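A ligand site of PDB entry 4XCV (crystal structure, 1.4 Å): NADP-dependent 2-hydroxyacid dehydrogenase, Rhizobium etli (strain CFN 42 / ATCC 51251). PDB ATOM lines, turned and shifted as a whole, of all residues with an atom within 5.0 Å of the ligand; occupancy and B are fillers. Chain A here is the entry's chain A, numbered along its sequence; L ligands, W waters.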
ATOM      1  N   ALA A  75     -10.398  -5.000  18.057  1.00  0.00           N
ATOM      2  CA  ALA A  75      -9.471  -4.487  19.031  1.00  0.00           C
ATOM      3  C   ALA A  75      -8.936  -3.132  18.628  1.00  0.00           C
ATOM      4  O   ALA A  75      -8.473  -2.344  19.474  1.00  0.00           O
ATOM      5  CB  ALA A  75      -8.310  -5.466  19.230  1.00  0.00           C
ATOM      6  N   GLY A  76      -8.923  -2.881  17.324  1.00  0.00           N
ATOM      7  CA  GLY A  76      -8.477  -1.622  16.772  1.00  0.00           C
ATOM      8  C   GLY A  76      -9.666  -0.698  16.496  1.00  0.00           C
ATOM      9  O   GLY A  76     -10.826  -1.131  16.389  1.00  0.00           O
ATOM     10  N   ARG A  93     -13.563   0.099  22.723  1.00  0.00           N
ATOM     11  CA  ARG A  93     -12.863  -0.917  21.947  1.00  0.00           C
ATOM     12  C   ARG A  93     -13.072  -2.299  22.501  1.00  0.00           C
ATOM     13  O   ARG A  93     -13.479  -2.478  23.633  1.00  0.00           O
ATOM     14  CB  ARG A  93     -11.389  -0.585  21.780  1.00  0.00           C
ATOM     15  CG  ARG A  93     -10.635  -0.749  23.032  1.00  0.00           C
ATOM     16  CD  ARG A  93      -9.234  -0.182  22.823  1.00  0.00           C
ATOM     17  NE  ARG A  93      -8.354  -0.668  23.801  1.00  0.00           N
ATOM     18  CZ  ARG A  93      -7.536  -1.707  23.617  1.00  0.00           C
ATOM     19  NH1 ARG A  93      -7.440  -2.385  22.468  1.00  0.00           N
ATOM     20  NH2 ARG A  93      -6.828  -2.058  24.622  1.00  0.00           N
ATOM     21  N   LEU A  99      -8.301 -13.006  25.442  1.00  0.00           N
ATOM     22  CA  LEU A  99      -7.352 -12.898  24.386  1.00  0.00           C
ATOM     23  C   LEU A  99      -5.963 -12.457  24.836  1.00  0.00           C
ATOM     24  O   LEU A  99      -4.918 -12.714  24.186  1.00  0.00           O
ATOM     25  CB  LEU A  99      -7.862 -11.881  23.407  1.00  0.00           C
ATOM     26  CG  LEU A  99      -7.370 -12.125  22.021  1.00  0.00           C
ATOM     27  CD1 LEU A  99      -7.734 -13.570  21.626  1.00  0.00           C
ATOM     28  CD2 LEU A  99      -8.066 -11.090  21.155  1.00  0.00           C
ATOM     29  N   MET A 103      -2.237 -13.732  23.438  1.00  0.00           N
ATOM     30  CA  MET A 103      -1.183 -12.889  22.839  1.00  0.00           C
ATOM     31  C   MET A 103       0.088 -13.136  23.581  1.00  0.00           C
ATOM     32  O   MET A 103       1.168 -13.261  22.967  1.00  0.00           O
ATOM     33  CB  MET A 103      -1.536 -11.403  22.924  1.00  0.00           C
ATOM     34  CG  MET A 103      -0.430 -10.548  22.315  1.00  0.00           C
ATOM     35  SD  MET A 103      -0.045 -10.879  20.592  1.00  0.00           S
ATOM     36  CE  MET A 103      -1.307  -9.885  19.836  1.00  0.00           C
ATOM     37  N   GLY A 147       4.710  -0.528  23.580  1.00  0.00           N
ATOM     38  CA  GLY A 147       3.285  -0.614  23.903  1.00  0.00           C
ATOM     39  C   GLY A 147       3.165  -1.338  25.221  1.00  0.00           C
ATOM     40  O   GLY A 147       3.554  -2.518  25.338  1.00  0.00           O
ATOM     41  N   LEU A 148       2.668  -0.645  26.224  1.00  0.00           N
ATOM     42  CA  LEU A 148       2.543  -1.159  27.581  1.00  0.00           C
ATOM     43  C   LEU A 148       1.110  -1.023  28.014  1.00  0.00           C
ATOM     44  O   LEU A 148       0.813  -0.533  29.133  1.00  0.00           O
ATOM     45  CB  LEU A 148       3.502  -0.424  28.511  1.00  0.00           C
ATOM     46  CG  LEU A 148       4.971  -0.641  28.204  1.00  0.00           C
ATOM     47  CD1 LEU A 148       5.790   0.181  29.170  1.00  0.00           C
ATOM     48  CD2 LEU A 148       5.382  -2.135  28.232  1.00  0.00           C
ATOM     49  N   GLY A 149       0.192  -1.431  27.149  1.00  0.00           N
ATOM     50  CA  GLY A 149      -1.247  -1.387  27.455  1.00  0.00           C
ATOM     51  C   GLY A 149      -1.685  -2.752  27.969  1.00  0.00           C
ATOM     52  O   GLY A 149      -0.919  -3.456  28.654  1.00  0.00           O
ATOM     53  N   ILE A 150      -2.900  -3.137  27.652  1.00  0.00           N
ATOM     54  CA  ILE A 150      -3.424  -4.412  28.111  1.00  0.00           C
ATOM     55  C   ILE A 150      -2.503  -5.556  27.656  1.00  0.00           C
ATOM     56  O   ILE A 150      -2.100  -6.408  28.458  1.00  0.00           O
ATOM     57  CB  ILE A 150      -4.830  -4.617  27.582  1.00  0.00           C
ATOM     58  CG1 ILE A 150      -5.795  -3.544  28.123  1.00  0.00           C
ATOM     59  CG2 ILE A 150      -5.304  -6.020  27.853  1.00  0.00           C
ATOM     60  CD1 ILE A 150      -6.133  -3.619  29.566  1.00  0.00           C
ATOM     61  N   LEU A 151      -2.104  -5.542  26.383  1.00  0.00           N
ATOM     62  CA  LEU A 151      -1.299  -6.623  25.862  1.00  0.00           C
ATOM     63  C   LEU A 151       0.149  -6.508  26.316  1.00  0.00           C
ATOM     64  O   LEU A 151       0.721  -7.478  26.802  1.00  0.00           O
ATOM     65  CB  LEU A 151      -1.407  -6.698  24.339  1.00  0.00           C
ATOM     66  CG  LEU A 151      -2.788  -6.940  23.812  1.00  0.00           C
ATOM     67  CD1 LEU A 151      -2.758  -6.988  22.282  1.00  0.00           C
ATOM     68  CD2 LEU A 151      -3.447  -8.182  24.396  1.00  0.00           C
ATOM     69  N   GLY A 152       0.750  -5.336  26.227  1.00  0.00           N
ATOM     70  CA  GLY A 152       2.150  -5.229  26.562  1.00  0.00           C
ATOM     71  C   GLY A 152       2.435  -5.503  28.005  1.00  0.00           C
ATOM     72  O   GLY A 152       3.466  -6.094  28.316  1.00  0.00           O
ATOM     73  N   TRP A 169       8.538   0.662  26.507  1.00  0.00           N
ATOM     74  CA  TRP A 169       8.419   1.974  25.911  1.00  0.00           C
ATOM     75  C   TRP A 169       6.930   2.226  25.646  1.00  0.00           C
ATOM     76  O   TRP A 169       6.221   1.368  25.140  1.00  0.00           O
ATOM     77  CB  TRP A 169       9.232   2.014  24.619  1.00  0.00           C
ATOM     78  CG  TRP A 169       9.168   3.319  23.854  1.00  0.00           C
ATOM     79  CD1 TRP A 169       9.951   4.422  24.073  1.00  0.00           C
ATOM     80  CD2 TRP A 169       8.353   3.639  22.726  1.00  0.00           C
ATOM     81  NE1 TRP A 169       9.693   5.388  23.127  1.00  0.00           N
ATOM     82  CE2 TRP A 169       8.721   4.935  22.284  1.00  0.00           C
ATOM     83  CE3 TRP A 169       7.389   2.967  21.993  1.00  0.00           C
ATOM     84  CZ2 TRP A 169       8.143   5.552  21.169  1.00  0.00           C
ATOM     85  CZ3 TRP A 169       6.856   3.572  20.883  1.00  0.00           C
ATOM     86  CH2 TRP A 169       7.224   4.833  20.484  1.00  0.00           C
ATOM     87  N   SER A 170       6.485   3.421  25.986  1.00  0.00           N
ATOM     88  CA  SER A 170       5.085   3.831  25.749  1.00  0.00           C
ATOM     89  C   SER A 170       5.016   5.311  25.666  1.00  0.00           C
ATOM     90  O   SER A 170       5.998   6.005  25.899  1.00  0.00           O
ATOM     91  CB  SER A 170       4.159   3.270  26.810  1.00  0.00           C
ATOM     92  OG  SER A 170       4.556   3.598  28.119  1.00  0.00           O
ATOM     93  N   ARG A 171       3.868   5.836  25.288  1.00  0.00           N
ATOM     94  CA  ARG A 171       3.744   7.275  25.042  1.00  0.00           C
ATOM     95  C   ARG A 171       4.003   8.063  26.315  1.00  0.00           C
ATOM     96  O   ARG A 171       4.738   9.094  26.316  1.00  0.00           O
ATOM     97  CB  ARG A 171       2.349   7.557  24.433  1.00  0.00           C
ATOM     98  CG  ARG A 171       2.238   8.906  23.773  1.00  0.00           C
ATOM     99  CD  ARG A 171       0.947   9.010  22.933  1.00  0.00           C
ATOM    100  NE  ARG A 171      -0.278   8.917  23.744  1.00  0.00           N
ATOM    101  CZ  ARG A 171      -0.914   9.897  24.370  1.00  0.00           C
ATOM    102  NH1 ARG A 171      -0.480  11.143  24.308  1.00  0.00           N
ATOM    103  NH2 ARG A 171      -2.017   9.631  25.089  1.00  0.00           N
ATOM    104  N   THR A 172       3.385   7.638  27.391  1.00  0.00           N
ATOM    105  CA  THR A 172       3.669   8.104  28.746  1.00  0.00           C
ATOM    106  C   THR A 172       4.373   7.008  29.491  1.00  0.00           C
ATOM    107  O   THR A 172       3.931   5.861  29.500  1.00  0.00           O
ATOM    108  CB  THR A 172       2.360   8.476  29.474  1.00  0.00           C
ATOM    109  OG1 THR A 172       1.767   9.569  28.773  1.00  0.00           O
ATOM    110  CG2 THR A 172       2.610   8.907  30.881  1.00  0.00           C
ATOM    111  N   LYS A 174       5.425   4.279  31.968  1.00  0.00           N
ATOM    112  CA  LYS A 174       4.756   3.474  33.018  1.00  0.00           C
ATOM    113  C   LYS A 174       5.674   3.235  34.189  1.00  0.00           C
ATOM    114  O   LYS A 174       6.927   3.347  34.107  1.00  0.00           O
ATOM    115  CB  LYS A 174       4.385   2.116  32.469  1.00  0.00           C
ATOM    116  CG  LYS A 174       3.470   2.224  31.330  1.00  0.00           C
ATOM    117  CD  LYS A 174       2.107   2.742  31.708  1.00  0.00           C
ATOM    118  CE  LYS A 174       1.287   3.025  30.471  1.00  0.00           C
ATOM    119  NZ  LYS A 174       1.494   4.456  30.043  1.00  0.00           N
ATOM    120  N   ALA A 184       7.982   8.353  25.395  1.00  0.00           N
ATOM    121  CA  ALA A 184       7.955   8.507  23.927  1.00  0.00           C
ATOM    122  C   ALA A 184       9.306   9.010  23.351  1.00  0.00           C
ATOM    123  O   ALA A 184       9.890   8.379  22.485  1.00  0.00           O
ATOM    124  CB  ALA A 184       6.818   9.449  23.502  1.00  0.00           C
ATOM    125  N   LEU A 200       3.635  -4.044  20.133  1.00  0.00           N
ATOM    126  CA  LEU A 200       2.251  -4.180  20.581  1.00  0.00           C
ATOM    127  C   LEU A 200       1.609  -2.801  20.644  1.00  0.00           C
ATOM    128  O   LEU A 200       0.966  -2.415  21.640  1.00  0.00           O
ATOM    129  CB  LEU A 200       2.157  -4.905  21.934  1.00  0.00           C
ATOM    130  CG  LEU A 200       2.515  -6.396  21.890  1.00  0.00           C
ATOM    131  CD1 LEU A 200       2.694  -6.950  23.268  1.00  0.00           C
ATOM    132  CD2 LEU A 200       1.490  -7.198  21.108  1.00  0.00           C
ATOM    133  N   LEU A 201       1.781  -2.066  19.545  1.00  0.00           N
ATOM    134  CA  LEU A 201       1.231  -0.698  19.416  1.00  0.00           C
ATOM    135  C   LEU A 201      -0.078  -0.690  18.615  1.00  0.00           C
ATOM    136  O   LEU A 201      -0.218  -1.484  17.678  1.00  0.00           O
ATOM    137  CB  LEU A 201       2.227   0.222  18.696  1.00  0.00           C
ATOM    138  CG  LEU A 201       3.561   0.499  19.423  1.00  0.00           C
ATOM    139  CD1 LEU A 201       4.488   1.266  18.463  1.00  0.00           C
ATOM    140  CD2 LEU A 201       3.338   1.253  20.698  1.00  0.00           C
ATOM    141  N   PRO A 202      -1.000   0.224  18.916  1.00  0.00           N
ATOM    142  CA  PRO A 202      -2.116   0.492  17.997  1.00  0.00           C
ATOM    143  C   PRO A 202      -1.651   1.191  16.750  1.00  0.00           C
ATOM    144  O   PRO A 202      -0.518   1.743  16.719  1.00  0.00           O
ATOM    145  CB  PRO A 202      -3.032   1.421  18.803  1.00  0.00           C
ATOM    146  CG  PRO A 202      -2.146   2.055  19.817  1.00  0.00           C
ATOM    147  CD  PRO A 202      -0.896   1.228  19.978  1.00  0.00           C
ATOM    148  N   LEU A 203      -2.470   1.181  15.708  1.00  0.00           N
ATOM    149  CA  LEU A 203      -2.218   1.967  14.484  1.00  0.00           C
ATOM    150  C   LEU A 203      -2.845   3.328  14.625  1.00  0.00           C
ATOM    151  O   LEU A 203      -4.073   3.460  14.792  1.00  0.00           O
ATOM    152  CB  LEU A 203      -2.827   1.278  13.265  1.00  0.00           C
ATOM    153  CG  LEU A 203      -2.485   1.992  11.938  1.00  0.00           C
ATOM    154  CD1 LEU A 203      -1.015   1.920  11.625  1.00  0.00           C
ATOM    155  CD2 LEU A 203      -3.252   1.384  10.768  1.00  0.00           C
ATOM    156  N   THR A 204      -1.990   4.339  14.586  1.00  0.00           N
ATOM    157  CA  THR A 204      -2.377   5.742  14.565  1.00  0.00           C
ATOM    158  C   THR A 204      -1.526   6.398  13.502  1.00  0.00           C
ATOM    159  O   THR A 204      -0.549   5.822  13.037  1.00  0.00           O
ATOM    160  CB  THR A 204      -2.132   6.429  15.917  1.00  0.00           C
ATOM    161  OG1 THR A 204      -0.721   6.457  16.167  1.00  0.00           O
ATOM    162  CG2 THR A 204      -2.754   5.650  17.050  1.00  0.00           C
ATOM    163  N   GLU A 206       0.795   8.453  14.061  1.00  0.00           N
ATOM    164  CA  GLU A 206       2.146   8.449  14.579  1.00  0.00           C
ATOM    165  C   GLU A 206       2.835   7.091  14.531  1.00  0.00           C
ATOM    166  O   GLU A 206       4.057   7.016  14.472  1.00  0.00           O
ATOM    167  CB  GLU A 206       2.161   8.876  16.028  1.00  0.00           C
ATOM    168  CG  GLU A 206       1.876  10.314  16.317  1.00  0.00           C
ATOM    169  CD  GLU A 206       1.747  10.472  17.813  1.00  0.00           C
ATOM    170  OE1 GLU A 206       0.605  10.734  18.284  1.00  0.00           O
ATOM    171  OE2 GLU A 206       2.786  10.229  18.512  1.00  0.00           O
ATOM    172  N   THR A 207       2.073   6.010  14.521  1.00  0.00           N
ATOM    173  CA  THR A 207       2.687   4.707  14.425  1.00  0.00           C
ATOM    174  C   THR A 207       2.613   4.065  13.019  1.00  0.00           C
ATOM    175  O   THR A 207       2.947   2.888  12.836  1.00  0.00           O
ATOM    176  CB  THR A 207       2.102   3.736  15.450  1.00  0.00           C
ATOM    177  OG1 THR A 207       0.772   3.392  15.060  1.00  0.00           O
ATOM    178  CG2 THR A 207       2.096   4.283  16.868  1.00  0.00           C
ATOM    179  N   ALA A 233       3.127  -7.888  16.517  1.00  0.00           N
ATOM    180  CA  ALA A 233       1.741  -8.404  16.521  1.00  0.00           C
ATOM    181  C   ALA A 233       0.743  -7.322  16.801  1.00  0.00           C
ATOM    182  O   ALA A 233      -0.368  -7.601  17.234  1.00  0.00           O
ATOM    183  CB  ALA A 233       1.598  -9.555  17.537  1.00  0.00           C
ATOM    184  N   GLY A 234       1.099  -6.067  16.524  1.00  0.00           N
ATOM    185  CA  GLY A 234       0.175  -4.944  16.690  1.00  0.00           C
ATOM    186  C   GLY A 234      -0.637  -4.764  15.437  1.00  0.00           C
ATOM    187  O   GLY A 234      -1.669  -5.433  15.270  1.00  0.00           O
ATOM    188  N   ARG A 235      -0.155  -3.879  14.554  1.00  0.00           N
ATOM    189  CA  ARG A 235      -0.785  -3.650  13.278  1.00  0.00           C
ATOM    190  C   ARG A 235       0.255  -3.667  12.176  1.00  0.00           C
ATOM    191  O   ARG A 235       1.351  -3.135  12.313  1.00  0.00           O
ATOM    192  CB  ARG A 235      -1.540  -2.306  13.296  1.00  0.00           C
ATOM    193  CG  ARG A 235      -2.737  -2.264  14.254  1.00  0.00           C
ATOM    194  CD  ARG A 235      -3.951  -3.048  13.760  1.00  0.00           C
ATOM    195  NE  ARG A 235      -4.407  -2.498  12.500  1.00  0.00           N
ATOM    196  CZ  ARG A 235      -5.256  -1.480  12.358  1.00  0.00           C
ATOM    197  NH1 ARG A 235      -5.834  -0.897  13.402  1.00  0.00           N
ATOM    198  NH2 ARG A 235      -5.546  -1.071  11.125  1.00  0.00           N
ATOM    199  N   ASP A 259       2.984 -11.428  12.933  1.00  0.00           N
ATOM    200  CA  ASP A 259       1.609 -11.894  12.853  1.00  0.00           C
ATOM    201  C   ASP A 259       0.728 -10.974  12.032  1.00  0.00           C
ATOM    202  O   ASP A 259      -0.432 -11.333  11.732  1.00  0.00           O
ATOM    203  CB  ASP A 259       0.975 -11.943  14.256  1.00  0.00           C
ATOM    204  CG  ASP A 259      -0.364 -12.620  14.280  1.00  0.00           C
ATOM    205  OD1 ASP A 259      -0.483 -13.816  13.901  1.00  0.00           O
ATOM    206  OD2 ASP A 259      -1.355 -12.005  14.751  1.00  0.00           O
ATOM    207  N   VAL A 260       1.239  -9.797  11.697  1.00  0.00           N
ATOM    208  CA  VAL A 260       0.467  -8.758  11.006  1.00  0.00           C
ATOM    209  C   VAL A 260       1.259  -8.201   9.861  1.00  0.00           C
ATOM    210  O   VAL A 260       2.462  -8.183   9.925  1.00  0.00           O
ATOM    211  CB  VAL A 260       0.023  -7.655  12.002  1.00  0.00           C
ATOM    212  CG1 VAL A 260      -0.915  -8.219  13.033  1.00  0.00           C
ATOM    213  CG2 VAL A 260       1.237  -7.019  12.686  1.00  0.00           C
ATOM    214  N   HIS A 283      -2.004 -13.679  11.052  1.00  0.00           N
ATOM    215  CA  HIS A 283      -2.914 -12.938  11.881  1.00  0.00           C
ATOM    216  C   HIS A 283      -3.808 -13.861  12.682  1.00  0.00           C
ATOM    217  O   HIS A 283      -5.007 -13.675  12.728  1.00  0.00           O
ATOM    218  CB  HIS A 283      -3.672 -11.877  11.063  1.00  0.00           C
ATOM    219  CG  HIS A 283      -4.158 -10.726  11.890  1.00  0.00           C
ATOM    220  ND1 HIS A 283      -4.408  -9.463  11.381  1.00  0.00           N
ATOM    221  CD2 HIS A 283      -4.403 -10.623  13.226  1.00  0.00           C
ATOM    222  CE1 HIS A 283      -4.832  -8.666  12.345  1.00  0.00           C
ATOM    223  NE2 HIS A 283      -4.842  -9.355  13.479  1.00  0.00           N
ATOM    224  N   ALA A 285      -2.461 -14.865  15.930  1.00  0.00           N
ATOM    225  CA  ALA A 285      -1.849 -14.857  17.301  1.00  0.00           C
ATOM    226  C   ALA A 285      -2.927 -14.733  18.373  1.00  0.00           C
ATOM    227  O   ALA A 285      -2.806 -15.335  19.446  1.00  0.00           O
ATOM    228  CB  ALA A 285      -0.900 -13.702  17.447  1.00  0.00           C
ATOM    229  N   ALA A 286      -3.953 -13.923  18.166  1.00  0.00           N
ATOM    230  CA  ALA A 286      -4.924 -13.655  19.191  1.00  0.00           C
ATOM    231  C   ALA A 286      -6.225 -13.232  18.495  1.00  0.00           C
ATOM    232  O   ALA A 286      -6.539 -12.089  18.443  1.00  0.00           O
ATOM    233  CB  ALA A 286      -4.427 -12.564  20.140  1.00  0.00           C
ATOM    234  N   VAL A 287      -6.886 -14.173  17.882  1.00  0.00           N
ATOM    235  CA  VAL A 287      -8.176 -13.926  17.243  1.00  0.00           C
ATOM    236  C   VAL A 287      -9.245 -14.406  18.197  1.00  0.00           C
ATOM    237  O   VAL A 287      -9.157 -15.508  18.773  1.00  0.00           O
ATOM    238  CB  VAL A 287      -8.281 -14.698  15.900  1.00  0.00           C
ATOM    239  CG1 VAL A 287      -9.730 -14.764  15.375  1.00  0.00           C
ATOM    240  CG2 VAL A 287      -7.347 -14.093  14.863  1.00  0.00           C
ATOM    241  N   TYR A 320      -6.473   6.394  20.023  1.00  0.00           N
ATOM    242  CA  TYR A 320      -6.479   4.979  20.389  1.00  0.00           C
ATOM    243  C   TYR A 320      -7.020   4.810  21.791  1.00  0.00           C
ATOM    244  O   TYR A 320      -7.210   5.848  22.499  1.00  0.00           O
ATOM    245  CB  TYR A 320      -5.037   4.386  20.280  1.00  0.00           C
ATOM    246  CG  TYR A 320      -4.090   4.926  21.301  1.00  0.00           C
ATOM    247  CD1 TYR A 320      -3.373   6.075  21.073  1.00  0.00           C
ATOM    248  CD2 TYR A 320      -3.912   4.268  22.503  1.00  0.00           C
ATOM    249  CE1 TYR A 320      -2.520   6.607  22.019  1.00  0.00           C
ATOM    250  CE2 TYR A 320      -3.085   4.769  23.478  1.00  0.00           C
ATOM    251  CZ  TYR A 320      -2.375   5.945  23.240  1.00  0.00           C
ATOM    252  OH  TYR A 320      -1.530   6.470  24.163  1.00  0.00           O
ATOM    253  OXT TYR A 320      -7.301   3.672  22.207  1.00  0.00           O
HETATM  254  P1  LIG L   1      -3.760  -0.344  24.630  1.00  0.00           P
HETATM  255  O1  LIG L   1      -4.146  -0.938  25.945  1.00  0.00           O
HETATM  256  O2  LIG L   1      -4.516   0.826  24.055  1.00  0.00           O
HETATM  257  O3  LIG L   1      -2.212   0.046  24.746  1.00  0.00           O
HETATM  258  C1  LIG L   1      -1.590   0.776  23.684  1.00  0.00           C
HETATM  259  C2  LIG L   1      -0.169   1.058  24.105  1.00  0.00           C
HETATM  260  O4  LIG L   1       0.494   1.668  23.001  1.00  0.00           O
HETATM  261  C3  LIG L   1      -0.105   2.006  25.278  1.00  0.00           C
HETATM  262  O5  LIG L   1       0.982   1.651  26.155  1.00  0.00           O
HETATM  263  C4  LIG L   1       0.177   3.318  24.572  1.00  0.00           C
HETATM  264  O6  LIG L   1       0.878   4.304  25.374  1.00  0.00           O
HETATM  265  C5  LIG L   1       1.095   2.848  23.450  1.00  0.00           C
HETATM  266  N1  LIG L   1       1.193   3.808  22.349  1.00  0.00           N
HETATM  267  C6  LIG L   1       0.164   4.230  21.588  1.00  0.00           C
HETATM  268  N2  LIG L   1       0.611   5.207  20.734  1.00  0.00           N
HETATM  269  C7  LIG L   1       1.929   5.398  21.032  1.00  0.00           C
HETATM  270  C8  LIG L   1       2.898   6.289  20.560  1.00  0.00           C
HETATM  271  N3  LIG L   1       2.641   7.139  19.565  1.00  0.00           N
HETATM  272  N4  LIG L   1       4.120   6.227  21.106  1.00  0.00           N
HETATM  273  C9  LIG L   1       4.401   5.339  22.082  1.00  0.00           C
HETATM  274  N5  LIG L   1       3.522   4.461  22.587  1.00  0.00           N
HETATM  275  C10 LIG L   1       2.294   4.528  22.023  1.00  0.00           C
HETATM  276  O7  LIG L   1      -3.746  -1.480  23.492  1.00  0.00           O
HETATM  277  P2  LIG L   1      -3.608  -3.077  23.637  1.00  0.00           P
HETATM  278  O8  LIG L   1      -2.371  -3.338  24.438  1.00  0.00           O
HETATM  279  O9  LIG L   1      -4.833  -3.668  24.138  1.00  0.00           O
HETATM  280  O10 LIG L   1      -3.453  -3.493  22.123  1.00  0.00           O
HETATM  281  C11 LIG L   1      -2.409  -2.946  21.308  1.00  0.00           C
HETATM  282  C12 LIG L   1      -2.787  -3.223  19.847  1.00  0.00           C
HETATM  283  O11 LIG L   1      -2.658  -4.607  19.564  1.00  0.00           O
HETATM  284  C13 LIG L   1      -4.218  -2.922  19.483  1.00  0.00           C
HETATM  285  O12 LIG L   1      -4.400  -1.527  19.174  1.00  0.00           O
HETATM  286  C14 LIG L   1      -4.485  -3.818  18.285  1.00  0.00           C
HETATM  287  O13 LIG L   1      -4.245  -3.068  17.064  1.00  0.00           O
HETATM  288  C15 LIG L   1      -3.425  -4.872  18.379  1.00  0.00           C
HETATM  289  N6  LIG L   1      -3.906  -6.258  18.505  1.00  0.00           N
HETATM  290  C16 LIG L   1      -3.450  -7.221  17.650  1.00  0.00           C
HETATM  291  C17 LIG L   1      -3.957  -8.486  17.683  1.00  0.00           C
HETATM  292  C18 LIG L   1      -3.469  -9.534  16.834  1.00  0.00           C
HETATM  293  O14 LIG L   1      -4.229 -10.523  16.670  1.00  0.00           O
HETATM  294  N7  LIG L   1      -2.285  -9.523  16.259  1.00  0.00           N
HETATM  295  C19 LIG L   1      -4.971  -8.844  18.694  1.00  0.00           C
HETATM  296  C20 LIG L   1      -5.348  -7.747  19.561  1.00  0.00           C
HETATM  297  C21 LIG L   1      -4.883  -6.515  19.464  1.00  0.00           C
HETATM  298  P3  LIG L   1       0.213   4.846  26.744  1.00  0.00           P
HETATM  299  O15 LIG L   1       1.060   6.014  27.142  1.00  0.00           O
HETATM  300  O16 LIG L   1      -1.215   5.218  26.394  1.00  0.00           O
HETATM  301  O17 LIG L   1       0.219   3.719  27.695  1.00  0.00           O
HETATM  302  O   HOH W   1      -3.386   3.823  27.324  1.00  0.00           O
HETATM  303  O   HOH W   2      -3.998 -12.657  15.561  1.00  0.00           O
HETATM  304  O   HOH W   3       0.242  -2.816  24.553  1.00  0.00           O
HETATM  305  O   HOH W   4      -6.152  -5.074  22.134  1.00  0.00           O
HETATM  306  O   HOH W   5      -6.568  -7.777  15.820  1.00  0.00           O
HETATM  307  O   HOH W   6      -8.110  -9.755  17.885  1.00  0.00           O
HETATM  308  O   HOH W   7      -4.387   0.249  28.364  1.00  0.00           O
HETATM  309  O   HOH W   8      -4.874  -0.429  16.140  1.00  0.00           O
HETATM  310  O   HOH W   9      -5.282   2.898  25.608  1.00  0.00           O
HETATM  311  O   HOH W  10      -1.586   2.137  28.886  1.00  0.00           O
HETATM  312  O   HOH W  11       5.753   8.306  20.140  1.00  0.00           O
HETATM  313  O   HOH W  12      -2.570   7.471  27.472  1.00  0.00           O
HETATM  314  O   HOH W  13       0.058   8.499  26.968  1.00  0.00           O
HETATM  315  O   HOH W  14      -0.129   7.123  18.746  1.00  0.00           O
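The side-chain carboxylate (OD2) of Asp 259 is in hydrogen-bond range of a nitrogen (N7) of the ligand, 3.0 Å away.
The backbone NH (N) of Gly 149 sits at hydrogen-bond distance from an oxygen (O5) of the ligand, 3.3 Å away.
An oxygen (O15) of the ligand is in hydrogen-bond range of the backbone NH (N) of Thr 172 (2.8 Å).
A nitrogen (N7) of the ligand lies within hydrogen-bond range of the backbone carbonyl oxygen (O) of Ala 233 (2.9 Å).
An oxygen (O17) of the ligand is in salt-bridge range of the side-chain amino group (NZ) of Lys 174 (2.8 Å).
An oxygen (O5) of the ligand is in hydrogen-bond range of the backbone NH (N) of Leu 148 (2.8 Å).
An oxygen (O9) of the ligand is in salt-bridge range of the guanidinium group of Arg 93 (2.6 Å).
The backbone NH (N) of Ile 150 sits at hydrogen-bond distance from an oxygen (O1) of the ligand, at 3.0 Å.
NE2 of His 283 sits close to O14 of the ligand (3.5 Å).
The side-chain hydroxyl of Tyr 320 sits at hydrogen-bond distance from an oxygen (O16) of the ligand (2.6 Å).
N of Leu 151 is in hydrogen-bond range of O8 of the ligand (3.0 Å).
The side-chain carboxylate (OE2) of Glu 206 lies within hydrogen-bond range of a nitrogen (N3) of the ligand.
N of Arg 171 lies within hydrogen-bond range of N5 of the ligand (3.1 Å).
N of Ala 184 lies within hydrogen-bond range of O of Arg 171, 3.5 Å away.
The side-chain hydroxyl (OG1) of Thr 207 sits at hydrogen-bond distance from the backbone carbonyl oxygen (O) of Pro 202.
O of Thr 172 lies within hydrogen-bond range of NZ of Lys 174 (2.9 Å).
The backbone carbonyl oxygen (O) of Ala 75 sits at hydrogen-bond distance from the guanidinium group (NH1) of Arg 93 (3.2 Å).
The side-chain hydroxyl (OH) of Tyr 320 lies within hydrogen-bond range of the guanidinium group (NE) of Arg 171.
N of His 283 is in hydrogen-bond range of O of Asp 259.
The side-chain carboxylate (OD1) of Asp 259 is in hydrogen-bond range of the backbone NH (N) of Ala 285, 3.0 Å away.
The backbone carbonyl oxygen (O) of Thr 172 is in hydrogen-bond range of the side-chain hydroxyl (OG) of Ser 170.
O of Ala 286 sits close to O14 of the ligand (3.3 Å).
Residues that only touch the ligand: Trp 169, Pro 202, Arg 235, Leu 200, Gly 234, Ser 170, Ala 75, Leu 201, Met 103, Gly 147, Val 260 and Thr 207.
Hydrophobic or aromatic side chains that line the ligand: Ala 75, Met 103, Ile 150, Leu 151, Trp 169, Leu 201, Pro 202, Val 260, His 283 and Tyr 320.
The nearest printed residue that does not touch the ligand is Gly 152 (4.1 Å).
Water W3 lies within hydrogen-bond range of O8 of the ligand (2.7 Å), N of Gly 149 (2.9 Å), O of Leu 200 (3.0 Å), N of Gly 152 (3.1 Å) and O of Gly 147 (3.4 Å).
Water W13 lies within hydrogen-bond range of an oxygen (O15) of the ligand (2.7 Å), the side-chain hydroxyl of Thr 172 (2.7 Å) and the guanidinium group of Arg 171 (3.0 Å).
Water W4 lies within hydrogen-bond range of an oxygen (O9) of the ligand (2.8 Å) and the guanidinium group of Arg 93 (3.0 Å).
Water W12 lies within hydrogen-bond range of O16 of the ligand (2.8 Å) and NH2 of Arg 171 (3.3 Å).
Water W14 bridges OG1 of Thr 204 (2.7 Å) and N2 of the ligand (2.9 Å).
Water W8 lies within hydrogen-bond range of an oxygen (O13) of the ligand (2.9 Å), the backbone NH of Leu 203 (2.9 Å) and the guanidinium group of Arg 235 (2.9 Å).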
